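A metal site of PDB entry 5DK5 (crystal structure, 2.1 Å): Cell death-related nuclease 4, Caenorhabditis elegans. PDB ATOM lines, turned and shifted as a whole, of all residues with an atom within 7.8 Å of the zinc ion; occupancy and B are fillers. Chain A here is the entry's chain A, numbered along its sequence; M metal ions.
The backbone NH (N) of Tyr 272 lies close to the side-chain sulfur (SG) of Cys 270, at 3.4 Å.
The backbone carbonyl oxygen of Lys 275 is in hydrogen-bond range of the backbone NH of Cys 270, at 2.9 Å.
SG of Cys 270 sits close to NH2 of Arg 146, at 3.7 Å.
SG of Cys 273 lies close to N of Lys 275, at 3.6 Å.
O of Cys 280 sits at hydrogen-bond distance from NH1 of Arg 146, 3.2 Å away.
Within 4 Å of the zinc ion: Cys 220, Cys 270, Cys 273 and Cys 280.
The zinc ion is bound by SG of Cys 280.
SG of Cys 273 binds the zinc ion (2.3 Å).
The zinc ion is bound by the side-chain sulfur (SG) of Cys 270, 2.3 Å away.
The zinc ion is bound by SG of Cys 220 (2.4 Å).
The zinc ion has four donor atoms within binding distance.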
ATOM      1  N   ARG A 146     -19.608 -25.259 -11.658  1.00  0.00           N
ATOM      2  CA  ARG A 146     -19.547 -25.415 -13.105  1.00  0.00           C
ATOM      3  C   ARG A 146     -20.570 -26.442 -13.608  1.00  0.00           C
ATOM      4  O   ARG A 146     -20.606 -26.789 -14.788  1.00  0.00           O
ATOM      5  CB  ARG A 146     -18.133 -25.812 -13.528  1.00  0.00           C
ATOM      6  CG  ARG A 146     -17.135 -24.672 -13.385  1.00  0.00           C
ATOM      7  CD  ARG A 146     -15.769 -25.005 -13.960  1.00  0.00           C
ATOM      8  NE  ARG A 146     -15.855 -25.396 -15.369  1.00  0.00           N
ATOM      9  CZ  ARG A 146     -14.823 -25.434 -16.206  1.00  0.00           C
ATOM     10  NH1 ARG A 146     -13.611 -25.096 -15.785  1.00  0.00           N
ATOM     11  NH2 ARG A 146     -15.002 -25.800 -17.466  1.00  0.00           N
ATOM     12  N   LEU A 218     -20.822 -25.320 -17.213  1.00  0.00           N
ATOM     13  CA  LEU A 218     -19.929 -24.245 -17.631  1.00  0.00           C
ATOM     14  C   LEU A 218     -18.702 -24.823 -18.336  1.00  0.00           C
ATOM     15  O   LEU A 218     -18.018 -25.711 -17.820  1.00  0.00           O
ATOM     16  CB  LEU A 218     -19.511 -23.386 -16.422  1.00  0.00           C
ATOM     17  CG  LEU A 218     -20.659 -22.673 -15.693  1.00  0.00           C
ATOM     18  CD1 LEU A 218     -20.090 -21.757 -14.623  1.00  0.00           C
ATOM     19  CD2 LEU A 218     -21.549 -21.895 -16.645  1.00  0.00           C
ATOM     20  N   THR A 219     -18.441 -24.282 -19.526  1.00  0.00           N
ATOM     21  CA  THR A 219     -17.471 -24.838 -20.462  1.00  0.00           C
ATOM     22  C   THR A 219     -16.485 -23.761 -20.905  1.00  0.00           C
ATOM     23  O   THR A 219     -16.817 -22.578 -20.912  1.00  0.00           O
ATOM     24  CB  THR A 219     -18.189 -25.446 -21.683  1.00  0.00           C
ATOM     25  OG1 THR A 219     -18.834 -26.662 -21.292  1.00  0.00           O
ATOM     26  CG2 THR A 219     -17.230 -25.736 -22.818  1.00  0.00           C
ATOM     27  N   CYS A 220     -15.272 -24.166 -21.293  1.00  0.00           N
ATOM     28  CA  CYS A 220     -14.209 -23.206 -21.576  1.00  0.00           C
ATOM     29  C   CYS A 220     -14.259 -22.618 -23.004  1.00  0.00           C
ATOM     30  O   CYS A 220     -13.812 -21.492 -23.215  1.00  0.00           O
ATOM     31  CB  CYS A 220     -12.839 -23.848 -21.340  1.00  0.00           C
ATOM     32  SG  CYS A 220     -12.486 -25.299 -22.369  1.00  0.00           S
ATOM     33  N   CYS A 221     -14.791 -23.375 -23.953  1.00  0.00           N
ATOM     34  CA  CYS A 221     -14.857 -22.929 -25.337  1.00  0.00           C
ATOM     35  C   CYS A 221     -16.221 -23.191 -25.978  1.00  0.00           C
ATOM     36  O   CYS A 221     -16.921 -24.134 -25.611  1.00  0.00           O
ATOM     37  CB  CYS A 221     -13.774 -23.606 -26.179  1.00  0.00           C
ATOM     38  SG  CYS A 221     -12.086 -23.138 -25.741  1.00  0.00           S
ATOM     39  N   LEU A 252     -15.932 -18.687 -19.083  1.00  0.00           N
ATOM     40  CA  LEU A 252     -16.726 -19.904 -19.192  1.00  0.00           C
ATOM     41  C   LEU A 252     -18.096 -19.637 -19.795  1.00  0.00           C
ATOM     42  O   LEU A 252     -18.737 -18.633 -19.504  1.00  0.00           O
ATOM     43  CB  LEU A 252     -16.891 -20.582 -17.829  1.00  0.00           C
ATOM     44  CG  LEU A 252     -15.599 -20.961 -17.110  1.00  0.00           C
ATOM     45  CD1 LEU A 252     -15.909 -21.673 -15.808  1.00  0.00           C
ATOM     46  CD2 LEU A 252     -14.715 -21.840 -17.998  1.00  0.00           C
ATOM     47  N   VAL A 269     -15.093 -32.412 -14.733  1.00  0.00           N
ATOM     48  CA  VAL A 269     -14.490 -32.542 -16.065  1.00  0.00           C
ATOM     49  C   VAL A 269     -15.227 -31.678 -17.090  1.00  0.00           C
ATOM     50  O   VAL A 269     -16.445 -31.780 -17.258  1.00  0.00           O
ATOM     51  CB  VAL A 269     -14.461 -34.021 -16.517  1.00  0.00           C
ATOM     52  CG1 VAL A 269     -15.767 -34.718 -16.190  1.00  0.00           C
ATOM     53  CG2 VAL A 269     -14.118 -34.137 -18.003  1.00  0.00           C
ATOM     54  N   CYS A 270     -14.475 -30.821 -17.787  1.00  0.00           N
ATOM     55  CA  CYS A 270     -15.037 -29.915 -18.784  1.00  0.00           C
ATOM     56  C   CYS A 270     -15.583 -30.703 -19.976  1.00  0.00           C
ATOM     57  O   CYS A 270     -14.929 -31.614 -20.472  1.00  0.00           O
ATOM     58  CB  CYS A 270     -13.953 -28.917 -19.242  1.00  0.00           C
ATOM     59  SG  CYS A 270     -14.465 -27.792 -20.566  1.00  0.00           S
ATOM     60  N   ARG A 271     -16.783 -30.345 -20.424  1.00  0.00           N
ATOM     61  CA  ARG A 271     -17.429 -31.061 -21.524  1.00  0.00           C
ATOM     62  C   ARG A 271     -16.722 -30.826 -22.859  1.00  0.00           C
ATOM     63  O   ARG A 271     -16.869 -31.638 -23.777  1.00  0.00           O
ATOM     64  CB  ARG A 271     -18.897 -30.642 -21.631  1.00  0.00           C
ATOM     65  CG  ARG A 271     -19.743 -30.995 -20.421  1.00  0.00           C
ATOM     66  CD  ARG A 271     -20.235 -32.436 -20.467  1.00  0.00           C
ATOM     67  NE  ARG A 271     -19.157 -33.414 -20.301  1.00  0.00           N
ATOM     68  CZ  ARG A 271     -18.588 -33.720 -19.132  1.00  0.00           C
ATOM     69  NH1 ARG A 271     -18.985 -33.111 -18.016  1.00  0.00           N
ATOM     70  NH2 ARG A 271     -17.621 -34.625 -19.082  1.00  0.00           N
ATOM     71  N   TYR A 272     -15.989 -29.733 -22.969  1.00  0.00           N
ATOM     72  CA  TYR A 272     -15.295 -29.417 -24.217  1.00  0.00           C
ATOM     73  C   TYR A 272     -13.907 -30.057 -24.278  1.00  0.00           C
ATOM     74  O   TYR A 272     -13.665 -30.945 -25.091  1.00  0.00           O
ATOM     75  CB  TYR A 272     -15.175 -27.896 -24.395  1.00  0.00           C
ATOM     76  CG  TYR A 272     -14.515 -27.498 -25.697  1.00  0.00           C
ATOM     77  CD1 TYR A 272     -15.259 -27.426 -26.872  1.00  0.00           C
ATOM     78  CD2 TYR A 272     -13.166 -27.208 -25.759  1.00  0.00           C
ATOM     79  CE1 TYR A 272     -14.669 -27.070 -28.064  1.00  0.00           C
ATOM     80  CE2 TYR A 272     -12.562 -26.854 -26.950  1.00  0.00           C
ATOM     81  CZ  TYR A 272     -13.314 -26.785 -28.103  1.00  0.00           C
ATOM     82  OH  TYR A 272     -12.731 -26.430 -29.302  1.00  0.00           O
ATOM     83  N   CYS A 273     -13.001 -29.601 -23.414  1.00  0.00           N
ATOM     84  CA  CYS A 273     -11.620 -30.057 -23.457  1.00  0.00           C
ATOM     85  C   CYS A 273     -11.415 -31.399 -22.749  1.00  0.00           C
ATOM     86  O   CYS A 273     -10.342 -32.001 -22.837  1.00  0.00           O
ATOM     87  CB  CYS A 273     -10.695 -29.005 -22.841  1.00  0.00           C
ATOM     88  SG  CYS A 273     -11.019 -28.675 -21.095  1.00  0.00           S
ATOM     89  N   ARG A 274     -12.443 -31.850 -22.030  1.00  0.00           N
ATOM     90  CA  ARG A 274     -12.411 -33.147 -21.339  1.00  0.00           C
ATOM     91  C   ARG A 274     -11.393 -33.189 -20.207  1.00  0.00           C
ATOM     92  O   ARG A 274     -11.127 -34.257 -19.643  1.00  0.00           O
ATOM     93  CB  ARG A 274     -12.108 -34.275 -22.332  1.00  0.00           C
ATOM     94  CG  ARG A 274     -12.847 -34.188 -23.661  1.00  0.00           C
ATOM     95  CD  ARG A 274     -14.346 -34.011 -23.472  1.00  0.00           C
ATOM     96  NE  ARG A 274     -14.925 -35.017 -22.577  1.00  0.00           N
ATOM     97  CZ  ARG A 274     -16.222 -35.279 -22.473  1.00  0.00           C
ATOM     98  NH1 ARG A 274     -17.104 -34.604 -23.209  1.00  0.00           N
ATOM     99  NH2 ARG A 274     -16.643 -36.216 -21.639  1.00  0.00           N
ATOM    100  N   LYS A 275     -10.837 -32.039 -19.851  1.00  0.00           N
ATOM    101  CA  LYS A 275      -9.820 -31.969 -18.798  1.00  0.00           C
ATOM    102  C   LYS A 275     -10.469 -31.740 -17.436  1.00  0.00           C
ATOM    103  O   LYS A 275     -11.626 -31.316 -17.343  1.00  0.00           O
ATOM    104  CB  LYS A 275      -8.819 -30.853 -19.076  1.00  0.00           C
ATOM    105  CG  LYS A 275      -7.959 -31.088 -20.307  1.00  0.00           C
ATOM    106  CD  LYS A 275      -7.028 -29.906 -20.567  1.00  0.00           C
ATOM    107  CE  LYS A 275      -6.154 -30.137 -21.785  1.00  0.00           C
ATOM    108  NZ  LYS A 275      -5.341 -28.933 -22.116  1.00  0.00           N
ATOM    109  N   GLY A 276      -9.717 -32.006 -16.378  1.00  0.00           N
ATOM    110  CA  GLY A 276     -10.174 -31.721 -15.037  1.00  0.00           C
ATOM    111  C   GLY A 276     -10.325 -30.223 -14.840  1.00  0.00           C
ATOM    112  O   GLY A 276      -9.570 -29.447 -15.424  1.00  0.00           O
ATOM    113  N   MET A 277     -11.282 -29.820 -14.020  1.00  0.00           N
ATOM    114  CA  MET A 277     -11.555 -28.395 -13.799  1.00  0.00           C
ATOM    115  C   MET A 277     -10.539 -27.767 -12.849  1.00  0.00           C
ATOM    116  O   MET A 277     -10.730 -26.659 -12.362  1.00  0.00           O
ATOM    117  CB  MET A 277     -12.973 -28.218 -13.271  1.00  0.00           C
ATOM    118  CG  MET A 277     -14.035 -28.504 -14.324  1.00  0.00           C
ATOM    119  SD  MET A 277     -15.705 -28.660 -13.675  1.00  0.00           S
ATOM    120  CE  MET A 277     -16.622 -28.916 -15.192  1.00  0.00           C
ATOM    121  N   VAL A 279      -7.344 -27.933 -14.153  1.00  0.00           N
ATOM    122  CA  VAL A 279      -6.530 -27.463 -15.266  1.00  0.00           C
ATOM    123  C   VAL A 279      -7.336 -26.501 -16.135  1.00  0.00           C
ATOM    124  O   VAL A 279      -6.862 -25.406 -16.470  1.00  0.00           O
ATOM    125  CB  VAL A 279      -6.020 -28.638 -16.130  1.00  0.00           C
ATOM    126  CG1 VAL A 279      -5.300 -28.137 -17.383  1.00  0.00           C
ATOM    127  CG2 VAL A 279      -5.084 -29.525 -15.308  1.00  0.00           C
ATOM    128  N   CYS A 280      -8.535 -26.906 -16.498  1.00  0.00           N
ATOM    129  CA  CYS A 280      -9.441 -26.057 -17.257  1.00  0.00           C
ATOM    130  C   CYS A 280     -10.025 -24.977 -16.355  1.00  0.00           C
ATOM    131  O   CYS A 280     -10.427 -25.248 -15.230  1.00  0.00           O
ATOM    132  CB  CYS A 280     -10.561 -26.880 -17.887  1.00  0.00           C
ATOM    133  SG  CYS A 280     -11.858 -25.895 -18.658  1.00  0.00           S
ATOM    134  N   GLY A 281     -10.060 -23.738 -16.858  1.00  0.00           N
ATOM    135  CA  GLY A 281     -10.565 -22.608 -16.106  1.00  0.00           C
ATOM    136  C   GLY A 281      -9.439 -21.744 -15.548  1.00  0.00           C
ATOM    137  O   GLY A 281      -9.676 -20.817 -14.776  1.00  0.00           O
ATOM    138  N   GLN A 285      -9.938 -18.756 -22.799  1.00  0.00           N
ATOM    139  CA  GLN A 285      -9.496 -19.425 -24.023  1.00  0.00           C
ATOM    140  C   GLN A 285      -9.961 -18.708 -25.290  1.00  0.00           C
ATOM    141  O   GLN A 285      -9.496 -19.024 -26.386  1.00  0.00           O
ATOM    142  CB  GLN A 285      -9.990 -20.877 -24.037  1.00  0.00           C
ATOM    143  CG  GLN A 285      -9.468 -21.733 -22.892  1.00  0.00           C
ATOM    144  CD  GLN A 285      -7.963 -21.829 -22.884  1.00  0.00           C
ATOM    145  OE1 GLN A 285      -7.346 -22.235 -23.874  1.00  0.00           O
ATOM    146  NE2 GLN A 285      -7.341 -21.462 -21.766  1.00  0.00           N
HETATM  147 ZN    ZN M   1     -12.351 -26.888 -20.638  1.00  0.00          ZN
